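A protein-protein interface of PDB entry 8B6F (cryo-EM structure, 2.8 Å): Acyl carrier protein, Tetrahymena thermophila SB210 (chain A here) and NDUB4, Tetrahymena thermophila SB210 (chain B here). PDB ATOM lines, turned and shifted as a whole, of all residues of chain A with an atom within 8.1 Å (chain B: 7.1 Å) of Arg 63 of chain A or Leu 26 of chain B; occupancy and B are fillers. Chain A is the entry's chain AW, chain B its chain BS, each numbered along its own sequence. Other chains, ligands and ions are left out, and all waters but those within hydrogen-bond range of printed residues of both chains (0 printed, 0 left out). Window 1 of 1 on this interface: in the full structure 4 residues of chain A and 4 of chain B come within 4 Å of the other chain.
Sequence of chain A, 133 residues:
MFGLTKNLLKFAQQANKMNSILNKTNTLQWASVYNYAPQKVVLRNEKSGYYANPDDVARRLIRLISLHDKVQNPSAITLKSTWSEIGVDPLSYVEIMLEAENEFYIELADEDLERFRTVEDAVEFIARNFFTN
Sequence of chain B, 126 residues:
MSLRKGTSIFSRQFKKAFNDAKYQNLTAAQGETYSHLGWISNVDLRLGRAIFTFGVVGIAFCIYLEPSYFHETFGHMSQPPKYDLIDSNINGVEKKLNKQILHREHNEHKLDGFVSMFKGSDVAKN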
ATOM      1  N   ASP A  55     -31.887   9.581  -3.666  1.00  0.00           N
ATOM      2  CA  ASP A  55     -32.662  10.758  -4.041  1.00  0.00           C
ATOM      3  C   ASP A  55     -32.471  11.876  -3.022  1.00  0.00           C
ATOM      4  O   ASP A  55     -32.233  13.032  -3.388  1.00  0.00           O
ATOM      5  CB  ASP A  55     -34.139  10.390  -4.172  1.00  0.00           C
ATOM      6  CG  ASP A  55     -34.946  11.456  -4.883  1.00  0.00           C
ATOM      7  OD1 ASP A  55     -34.530  12.633  -4.862  1.00  0.00           O
ATOM      8  OD2 ASP A  55     -35.997  11.118  -5.465  1.00  0.00           O
ATOM      9  N   ASP A  56     -32.570  11.545  -1.733  1.00  0.00           N
ATOM     10  CA  ASP A  56     -32.356  12.550  -0.696  1.00  0.00           C
ATOM     11  C   ASP A  56     -30.929  13.077  -0.731  1.00  0.00           C
ATOM     12  O   ASP A  56     -30.699  14.280  -0.557  1.00  0.00           O
ATOM     13  CB  ASP A  56     -32.680  11.966   0.677  1.00  0.00           C
ATOM     14  CG  ASP A  56     -34.153  11.652   0.844  1.00  0.00           C
ATOM     15  OD1 ASP A  56     -34.984  12.357   0.232  1.00  0.00           O
ATOM     16  OD2 ASP A  56     -34.483  10.703   1.584  1.00  0.00           O
ATOM     17  N   VAL A  57     -29.956  12.193  -0.948  1.00  0.00           N
ATOM     18  CA  VAL A  57     -28.564  12.626  -1.026  1.00  0.00           C
ATOM     19  C   VAL A  57     -28.386  13.615  -2.171  1.00  0.00           C
ATOM     20  O   VAL A  57     -27.749  14.662  -2.019  1.00  0.00           O
ATOM     21  CB  VAL A  57     -27.630  11.410  -1.178  1.00  0.00           C
ATOM     22  CG1 VAL A  57     -26.207  11.851  -1.498  1.00  0.00           C
ATOM     23  CG2 VAL A  57     -27.650  10.566   0.083  1.00  0.00           C
ATOM     24  N   ALA A  58     -28.942  13.290  -3.339  1.00  0.00           N
ATOM     25  CA  ALA A  58     -28.804  14.175  -4.490  1.00  0.00           C
ATOM     26  C   ALA A  58     -29.470  15.521  -4.243  1.00  0.00           C
ATOM     27  O   ALA A  58     -28.910  16.569  -4.586  1.00  0.00           O
ATOM     28  CB  ALA A  58     -29.398  13.511  -5.730  1.00  0.00           C
ATOM     29  N   ARG A  59     -30.669  15.516  -3.663  1.00  0.00           N
ATOM     30  CA  ARG A  59     -31.363  16.776  -3.420  1.00  0.00           C
ATOM     31  C   ARG A  59     -30.614  17.636  -2.412  1.00  0.00           C
ATOM     32  O   ARG A  59     -30.476  18.847  -2.605  1.00  0.00           O
ATOM     33  CB  ARG A  59     -32.788  16.501  -2.950  1.00  0.00           C
ATOM     34  CG  ARG A  59     -33.649  15.893  -4.040  1.00  0.00           C
ATOM     35  CD  ARG A  59     -35.095  15.739  -3.618  1.00  0.00           C
ATOM     36  NE  ARG A  59     -35.898  15.206  -4.712  1.00  0.00           N
ATOM     37  CZ  ARG A  59     -36.385  15.931  -5.709  1.00  0.00           C
ATOM     38  NH1 ARG A  59     -36.190  17.238  -5.775  1.00  0.00           N
ATOM     39  NH2 ARG A  59     -37.081  15.330  -6.668  1.00  0.00           N
ATOM     40  N   ARG A  60     -30.111  17.027  -1.337  1.00  0.00           N
ATOM     41  CA  ARG A  60     -29.344  17.788  -0.359  1.00  0.00           C
ATOM     42  C   ARG A  60     -28.067  18.349  -0.969  1.00  0.00           C
ATOM     43  O   ARG A  60     -27.695  19.496  -0.700  1.00  0.00           O
ATOM     44  CB  ARG A  60     -29.029  16.913   0.853  1.00  0.00           C
ATOM     45  CG  ARG A  60     -30.232  16.677   1.751  1.00  0.00           C
ATOM     46  CD  ARG A  60     -30.080  15.423   2.591  1.00  0.00           C
ATOM     47  NE  ARG A  60     -28.942  15.493   3.499  1.00  0.00           N
ATOM     48  CZ  ARG A  60     -28.591  14.521   4.329  1.00  0.00           C
ATOM     49  NH1 ARG A  60     -29.271  13.388   4.395  1.00  0.00           N
ATOM     50  NH2 ARG A  60     -27.531  14.688   5.112  1.00  0.00           N
ATOM     51  N   LEU A  61     -27.377  17.557  -1.793  1.00  0.00           N
ATOM     52  CA  LEU A  61     -26.163  18.053  -2.432  1.00  0.00           C
ATOM     53  C   LEU A  61     -26.467  19.202  -3.386  1.00  0.00           C
ATOM     54  O   LEU A  61     -25.704  20.172  -3.463  1.00  0.00           O
ATOM     55  CB  LEU A  61     -25.457  16.917  -3.172  1.00  0.00           C
ATOM     56  CG  LEU A  61     -24.108  17.268  -3.808  1.00  0.00           C
ATOM     57  CD1 LEU A  61     -23.109  17.755  -2.771  1.00  0.00           C
ATOM     58  CD2 LEU A  61     -23.549  16.076  -4.560  1.00  0.00           C
ATOM     59  N   ILE A  62     -27.573  19.112  -4.126  1.00  0.00           N
ATOM     60  CA  ILE A  62     -27.934  20.184  -5.049  1.00  0.00           C
ATOM     61  C   ILE A  62     -28.292  21.451  -4.284  1.00  0.00           C
ATOM     62  O   ILE A  62     -27.948  22.562  -4.704  1.00  0.00           O
ATOM     63  CB  ILE A  62     -29.070  19.737  -5.983  1.00  0.00           C
ATOM     64  CG1 ILE A  62     -28.552  18.665  -6.938  1.00  0.00           C
ATOM     65  CG2 ILE A  62     -29.595  20.922  -6.785  1.00  0.00           C
ATOM     66  CD1 ILE A  62     -29.625  18.033  -7.744  1.00  0.00           C
ATOM     67  N   ARG A  63     -28.994  21.311  -3.158  1.00  0.00           N
ATOM     68  CA  ARG A  63     -29.287  22.480  -2.336  1.00  0.00           C
ATOM     69  C   ARG A  63     -28.001  23.106  -1.818  1.00  0.00           C
ATOM     70  O   ARG A  63     -27.850  24.332  -1.832  1.00  0.00           O
ATOM     71  CB  ARG A  63     -30.198  22.098  -1.170  1.00  0.00           C
ATOM     72  CG  ARG A  63     -31.595  21.660  -1.576  1.00  0.00           C
ATOM     73  CD  ARG A  63     -32.500  21.538  -0.358  1.00  0.00           C
ATOM     74  NE  ARG A  63     -33.724  20.799  -0.649  1.00  0.00           N
ATOM     75  CZ  ARG A  63     -33.898  19.503  -0.425  1.00  0.00           C
ATOM     76  NH1 ARG A  63     -32.942  18.755   0.101  1.00  0.00           N
ATOM     77  NH2 ARG A  63     -35.064  18.943  -0.733  1.00  0.00           N
ATOM     78  N   LEU A  64     -27.061  22.281  -1.360  1.00  0.00           N
ATOM     79  CA  LEU A  64     -25.789  22.812  -0.887  1.00  0.00           C
ATOM     80  C   LEU A  64     -25.063  23.551  -2.002  1.00  0.00           C
ATOM     81  O   LEU A  64     -24.500  24.629  -1.781  1.00  0.00           O
ATOM     82  CB  LEU A  64     -24.922  21.680  -0.341  1.00  0.00           C
ATOM     83  CG  LEU A  64     -23.559  22.094   0.215  1.00  0.00           C
ATOM     84  CD1 LEU A  64     -23.714  22.976   1.440  1.00  0.00           C
ATOM     85  CD2 LEU A  64     -22.737  20.868   0.540  1.00  0.00           C
ATOM     86  N   ILE A  65     -25.061  22.982  -3.209  1.00  0.00           N
ATOM     87  CA  ILE A  65     -24.417  23.637  -4.343  1.00  0.00           C
ATOM     88  C   ILE A  65     -25.106  24.959  -4.653  1.00  0.00           C
ATOM     89  O   ILE A  65     -24.448  25.978  -4.895  1.00  0.00           O
ATOM     90  CB  ILE A  65     -24.405  22.702  -5.567  1.00  0.00           C
ATOM     91  CG1 ILE A  65     -23.522  21.484  -5.297  1.00  0.00           C
ATOM     92  CG2 ILE A  65     -23.906  23.434  -6.806  1.00  0.00           C
ATOM     93  CD1 ILE A  65     -23.740  20.350  -6.270  1.00  0.00           C
ATOM     94  N   SER A  66     -26.440  24.968  -4.646  1.00  0.00           N
ATOM     95  CA  SER A  66     -27.168  26.196  -4.945  1.00  0.00           C
ATOM     96  C   SER A  66     -26.894  27.281  -3.913  1.00  0.00           C
ATOM     97  O   SER A  66     -26.943  28.472  -4.241  1.00  0.00           O
ATOM     98  CB  SER A  66     -28.666  25.904  -5.009  1.00  0.00           C
ATOM     99  OG  SER A  66     -28.946  24.913  -5.981  1.00  0.00           O
ATOM    100  N   LEU A  67     -26.613  26.898  -2.667  1.00  0.00           N
ATOM    101  CA  LEU A  67     -26.306  27.891  -1.644  1.00  0.00           C
ATOM    102  C   LEU A  67     -25.090  28.732  -2.016  1.00  0.00           C
ATOM    103  O   LEU A  67     -24.970  29.876  -1.563  1.00  0.00           O
ATOM    104  CB  LEU A  67     -26.075  27.204  -0.297  1.00  0.00           C
ATOM    105  CG  LEU A  67     -27.309  26.655   0.423  1.00  0.00           C
ATOM    106  CD1 LEU A  67     -26.901  25.950   1.704  1.00  0.00           C
ATOM    107  CD2 LEU A  67     -28.319  27.747   0.721  1.00  0.00           C
ATOM    108  N   HIS A  68     -24.188  28.193  -2.830  1.00  0.00           N
ATOM    109  CA  HIS A  68     -22.956  28.898  -3.151  1.00  0.00           C
ATOM    110  C   HIS A  68     -23.245  30.152  -3.969  1.00  0.00           C
ATOM    111  O   HIS A  68     -24.242  30.240  -4.688  1.00  0.00           O
ATOM    112  CB  HIS A  68     -22.003  27.982  -3.918  1.00  0.00           C
ATOM    113  CG  HIS A  68     -20.564  28.377  -3.804  1.00  0.00           C
ATOM    114  ND1 HIS A  68     -20.010  29.396  -4.548  1.00  0.00           N
ATOM    115  CD2 HIS A  68     -19.564  27.887  -3.036  1.00  0.00           C
ATOM    116  CE1 HIS A  68     -18.732  29.519  -4.239  1.00  0.00           C
ATOM    117  NE2 HIS A  68     -18.435  28.615  -3.324  1.00  0.00           N
ATOM    118  N   VAL A  71     -22.805  29.825  -7.988  1.00  0.00           N
ATOM    119  CA  VAL A  71     -23.928  29.169  -8.642  1.00  0.00           C
ATOM    120  C   VAL A  71     -25.038  30.186  -8.864  1.00  0.00           C
ATOM    121  O   VAL A  71     -25.462  30.881  -7.932  1.00  0.00           O
ATOM    122  CB  VAL A  71     -24.414  27.977  -7.805  1.00  0.00           C
ATOM    123  CG1 VAL A  71     -25.640  27.333  -8.435  1.00  0.00           C
ATOM    124  CG2 VAL A  71     -23.297  26.960  -7.651  1.00  0.00           C
ATOM    125  N   PRO A  74     -30.147  27.502  -9.902  1.00  0.00           N
ATOM    126  CA  PRO A  74     -30.332  26.148  -9.356  1.00  0.00           C
ATOM    127  C   PRO A  74     -31.087  25.220 -10.288  1.00  0.00           C
ATOM    128  O   PRO A  74     -30.894  24.001 -10.221  1.00  0.00           O
ATOM    129  CB  PRO A  74     -31.108  26.399  -8.056  1.00  0.00           C
ATOM    130  CG  PRO A  74     -30.790  27.800  -7.686  1.00  0.00           C
ATOM    131  CD  PRO A  74     -30.641  28.539  -8.980  1.00  0.00           C
ATOM    132  N   ILE A  77     -29.094  22.824 -12.666  1.00  0.00           N
ATOM    133  CA  ILE A  77     -28.271  21.772 -12.078  1.00  0.00           C
ATOM    134  C   ILE A  77     -28.991  20.437 -12.204  1.00  0.00           C
ATOM    135  O   ILE A  77     -30.146  20.296 -11.785  1.00  0.00           O
ATOM    136  CB  ILE A  77     -27.948  22.089 -10.610  1.00  0.00           C
ATOM    137  CG1 ILE A  77     -27.282  23.464 -10.501  1.00  0.00           C
ATOM    138  CG2 ILE A  77     -27.050  21.004 -10.023  1.00  0.00           C
ATOM    139  CD1 ILE A  77     -26.978  23.901  -9.081  1.00  0.00           C
ATOM    140  N   ILE A  96     -17.262  23.619  -1.527  1.00  0.00           N
ATOM    141  CA  ILE A  96     -18.547  22.930  -1.573  1.00  0.00           C
ATOM    142  C   ILE A  96     -18.405  21.510  -1.047  1.00  0.00           C
ATOM    143  O   ILE A  96     -19.296  20.990  -0.366  1.00  0.00           O
ATOM    144  CB  ILE A  96     -19.113  22.957  -3.004  1.00  0.00           C
ATOM    145  CG1 ILE A  96     -19.435  24.397  -3.411  1.00  0.00           C
ATOM    146  CG2 ILE A  96     -20.355  22.079  -3.108  1.00  0.00           C
ATOM    147  CD1 ILE A  96     -19.808  24.562  -4.869  1.00  0.00           C
ATOM    148  N   GLU A 103     -22.118  18.238   5.965  1.00  0.00           N
ATOM    149  CA  GLU A 103     -23.546  17.956   5.894  1.00  0.00           C
ATOM    150  C   GLU A 103     -23.824  16.462   5.994  1.00  0.00           C
ATOM    151  O   GLU A 103     -24.761  16.045   6.685  1.00  0.00           O
ATOM    152  CB  GLU A 103     -24.115  18.524   4.593  1.00  0.00           C
ATOM    153  CG  GLU A 103     -25.558  19.000   4.685  1.00  0.00           C
ATOM    154  CD  GLU A 103     -26.561  17.864   4.666  1.00  0.00           C
ATOM    155  OE1 GLU A 103     -26.163  16.718   4.380  1.00  0.00           O
ATOM    156  OE2 GLU A 103     -27.754  18.121   4.934  1.00  0.00           O
ATOM    157  N   ALA B  21     -37.912  30.861   9.677  1.00  0.00           N
ATOM    158  CA  ALA B  21     -36.875  30.527   8.712  1.00  0.00           C
ATOM    159  C   ALA B  21     -35.533  31.190   8.986  1.00  0.00           C
ATOM    160  O   ALA B  21     -34.588  30.965   8.225  1.00  0.00           O
ATOM    161  CB  ALA B  21     -37.339  30.903   7.300  1.00  0.00           C
ATOM    162  N   TYR B  23     -33.301  30.594  11.274  1.00  0.00           N
ATOM    163  CA  TYR B  23     -32.303  29.594  11.634  1.00  0.00           C
ATOM    164  C   TYR B  23     -32.641  28.222  11.059  1.00  0.00           C
ATOM    165  O   TYR B  23     -32.347  27.196  11.673  1.00  0.00           O
ATOM    166  CB  TYR B  23     -32.157  29.506  13.151  1.00  0.00           C
ATOM    167  CG  TYR B  23     -31.793  30.817  13.801  1.00  0.00           C
ATOM    168  CD1 TYR B  23     -30.507  31.327  13.703  1.00  0.00           C
ATOM    169  CD2 TYR B  23     -32.731  31.538  14.528  1.00  0.00           C
ATOM    170  CE1 TYR B  23     -30.166  32.521  14.299  1.00  0.00           C
ATOM    171  CE2 TYR B  23     -32.399  32.734  15.129  1.00  0.00           C
ATOM    172  CZ  TYR B  23     -31.114  33.218  15.011  1.00  0.00           C
ATOM    173  OH  TYR B  23     -30.772  34.408  15.606  1.00  0.00           O
ATOM    174  N   GLN B  24     -33.254  28.187   9.881  1.00  0.00           N
ATOM    175  CA  GLN B  24     -33.637  26.927   9.271  1.00  0.00           C
ATOM    176  C   GLN B  24     -32.427  26.237   8.647  1.00  0.00           C
ATOM    177  O   GLN B  24     -31.365  26.832   8.450  1.00  0.00           O
ATOM    178  CB  GLN B  24     -34.720  27.155   8.217  1.00  0.00           C
ATOM    179  CG  GLN B  24     -34.260  27.981   7.027  1.00  0.00           C
ATOM    180  CD  GLN B  24     -35.365  28.204   6.020  1.00  0.00           C
ATOM    181  OE1 GLN B  24     -36.416  27.569   6.084  1.00  0.00           O
ATOM    182  NE2 GLN B  24     -35.136  29.114   5.085  1.00  0.00           N
ATOM    183  N   ASN B  25     -32.600  24.954   8.341  1.00  0.00           N
ATOM    184  CA  ASN B  25     -31.592  24.155   7.650  1.00  0.00           C
ATOM    185  C   ASN B  25     -31.951  24.155   6.167  1.00  0.00           C
ATOM    186  O   ASN B  25     -32.842  23.422   5.732  1.00  0.00           O
ATOM    187  CB  ASN B  25     -31.546  22.741   8.220  1.00  0.00           C
ATOM    188  CG  ASN B  25     -30.469  21.890   7.585  1.00  0.00           C
ATOM    189  OD1 ASN B  25     -29.416  22.390   7.196  1.00  0.00           O
ATOM    190  ND2 ASN B  25     -30.729  20.595   7.472  1.00  0.00           N
ATOM    191  N   LEU B  26     -31.255  24.986   5.388  1.00  0.00           N
ATOM    192  CA  LEU B  26     -31.609  25.164   3.986  1.00  0.00           C
ATOM    193  C   LEU B  26     -31.376  23.911   3.153  1.00  0.00           C
ATOM    194  O   LEU B  26     -31.926  23.808   2.052  1.00  0.00           O
ATOM    195  CB  LEU B  26     -30.821  26.332   3.393  1.00  0.00           C
ATOM    196  CG  LEU B  26     -31.175  27.714   3.947  1.00  0.00           C
ATOM    197  CD1 LEU B  26     -30.204  28.764   3.441  1.00  0.00           C
ATOM    198  CD2 LEU B  26     -32.596  28.096   3.579  1.00  0.00           C
ATOM    199  N   THR B  27     -30.583  22.961   3.644  1.00  0.00           N
ATOM    200  CA  THR B  27     -30.331  21.733   2.903  1.00  0.00           C
ATOM    201  C   THR B  27     -31.444  20.705   3.062  1.00  0.00           C
ATOM    202  O   THR B  27     -31.406  19.671   2.388  1.00  0.00           O
ATOM    203  CB  THR B  27     -29.003  21.111   3.339  1.00  0.00           C
ATOM    204  OG1 THR B  27     -29.026  20.854   4.748  1.00  0.00           O
ATOM    205  CG2 THR B  27     -27.846  22.040   3.011  1.00  0.00           C
ATOM    206  N   ALA B  28     -32.419  20.956   3.928  1.00  0.00           N
ATOM    207  CA  ALA B  28     -33.523  20.037   4.157  1.00  0.00           C
ATOM    208  C   ALA B  28     -34.740  20.449   3.339  1.00  0.00           C
ATOM    209  O   ALA B  28     -34.883  21.602   2.926  1.00  0.00           O
ATOM    210  CB  ALA B  28     -33.886  19.987   5.643  1.00  0.00           C
ATOM    211  N   ALA B  29     -35.624  19.484   3.113  1.00  0.00           N
ATOM    212  CA  ALA B  29     -36.833  19.742   2.346  1.00  0.00           C
ATOM    213  C   ALA B  29     -37.761  20.683   3.104  1.00  0.00           C
ATOM    214  O   ALA B  29     -37.752  20.747   4.335  1.00  0.00           O
ATOM    215  CB  ALA B  29     -37.558  18.433   2.039  1.00  0.00           C
ATOM    216  N   GLN B  30     -38.571  21.423   2.349  1.00  0.00           N
ATOM    217  CA  GLN B  30     -39.530  22.330   2.963  1.00  0.00           C
ATOM    218  C   GLN B  30     -40.488  21.557   3.860  1.00  0.00           C
ATOM    219  O   GLN B  30     -40.921  20.449   3.530  1.00  0.00           O
ATOM    220  CB  GLN B  30     -40.307  23.090   1.889  1.00  0.00           C
ATOM    221  CG  GLN B  30     -39.454  24.059   1.093  1.00  0.00           C
ATOM    222  CD  GLN B  30     -40.248  24.803   0.041  1.00  0.00           C
ATOM    223  OE1 GLN B  30     -41.399  24.469  -0.236  1.00  0.00           O
ATOM    224  NE2 GLN B  30     -39.638  25.823  -0.551  1.00  0.00           N
ATOM    225  N   THR B  33     -37.393  21.694   7.550  1.00  0.00           N
ATOM    226  CA  THR B  33     -36.165  22.480   7.659  1.00  0.00           C
ATOM    227  C   THR B  33     -36.198  23.314   8.941  1.00  0.00           C
ATOM    228  O   THR B  33     -36.252  24.543   8.929  1.00  0.00           O
ATOM    229  CB  THR B  33     -35.981  23.355   6.419  1.00  0.00           C
ATOM    230  OG1 THR B  33     -34.849  24.215   6.601  1.00  0.00           O
ATOM    231  CG2 THR B  33     -37.219  24.206   6.146  1.00  0.00           C
ATOM    232  N   SER B  35     -34.262  23.376  12.951  1.00  0.00           N
ATOM    233  CA  SER B  35     -33.096  22.912  13.690  1.00  0.00           C
ATOM    234  C   SER B  35     -33.331  22.758  15.183  1.00  0.00           C
ATOM    235  O   SER B  35     -32.653  21.949  15.818  1.00  0.00           O
ATOM    236  CB  SER B  35     -31.928  23.886  13.483  1.00  0.00           C
ATOM    237  OG  SER B  35     -31.689  24.089  12.102  1.00  0.00           O
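The side-chain hydroxyl (OG1) of Thr 27 of chain B is in hydrogen-bond range of the side-chain carboxylate (OE2) of Glu 103 of chain A (3.0 Å). The backbone carbonyl oxygen (O) of Thr 27 of chain B lies within hydrogen-bond range of the guanidinium group (NH1) of Arg 63 of chain A.
The side-chain amide oxygen (OD1) of Asn 25 of chain B is in hydrogen-bond range of the side-chain hydroxyl (OG1) of Thr 27 of chain B. NH2 of Arg 60 of chain A is in salt-bridge range of OE1 of Glu 103 of chain A.
O of Thr 27 of chain B touches CG of Arg 60 of chain A, 3.3 Å away. O of Leu 26 of chain B touches CD of Arg 63 of chain A (3.4 Å). NE of Arg 63 of chain A touches O of Ala 28 of chain B (3.8 Å). Arg 63 of chain A touches Ala 29 of chain B. CD2 of Leu 67 of chain A touches CD1 of Leu 26 of chain B, at 3.5 Å.
Ala 58 of chain A touches none of the printed residues of chain B. Of the printed residues of chain B, Arg 60 of chain A touches Thr 27 (3.3 Å). Arg 63 of chain A touches just these residues of chain B: Leu 26, Thr 27, Ala 28 and Ala 29. Printed residues of chain B within 4 Å of Leu 67 of chain A: Leu 26. Pro 74 of chain A touches none of the printed residues of chain B. Printed residues of chain B within 4 Å of Glu 103 of chain A: Thr 27. Of chain A, only Arg 63 and Leu 67 come within 4 Å of Leu 26 of chain B. Of the printed residues of chain A, Ala 28 of chain B touches Arg 63. Of the printed residues of chain A, Ala 29 of chain B touches Arg 63. The nearest residue of chain B that does not touch Arg 63 of chain A is Gln 30 of chain B (5.3 Å). The nearest residue of chain A that does not touch Leu 26 of chain B is Leu 64 of chain A (6.1 Å).
Of the 11 printed residues of chain B, 4 touch a printed residue of chain A. Printed residues of chain B that touch a printed residue of chain A: Leu 26, Thr 27, Ala 28 and Ala 29. Of the 19 printed residues of chain A, 4 touch a printed residue of chain B. Printed residues of chain A that touch a printed residue of chain B: Arg 60, Arg 63, Leu 67 and Glu 103. Among the printed residues, 7 pairs touch across the chains.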
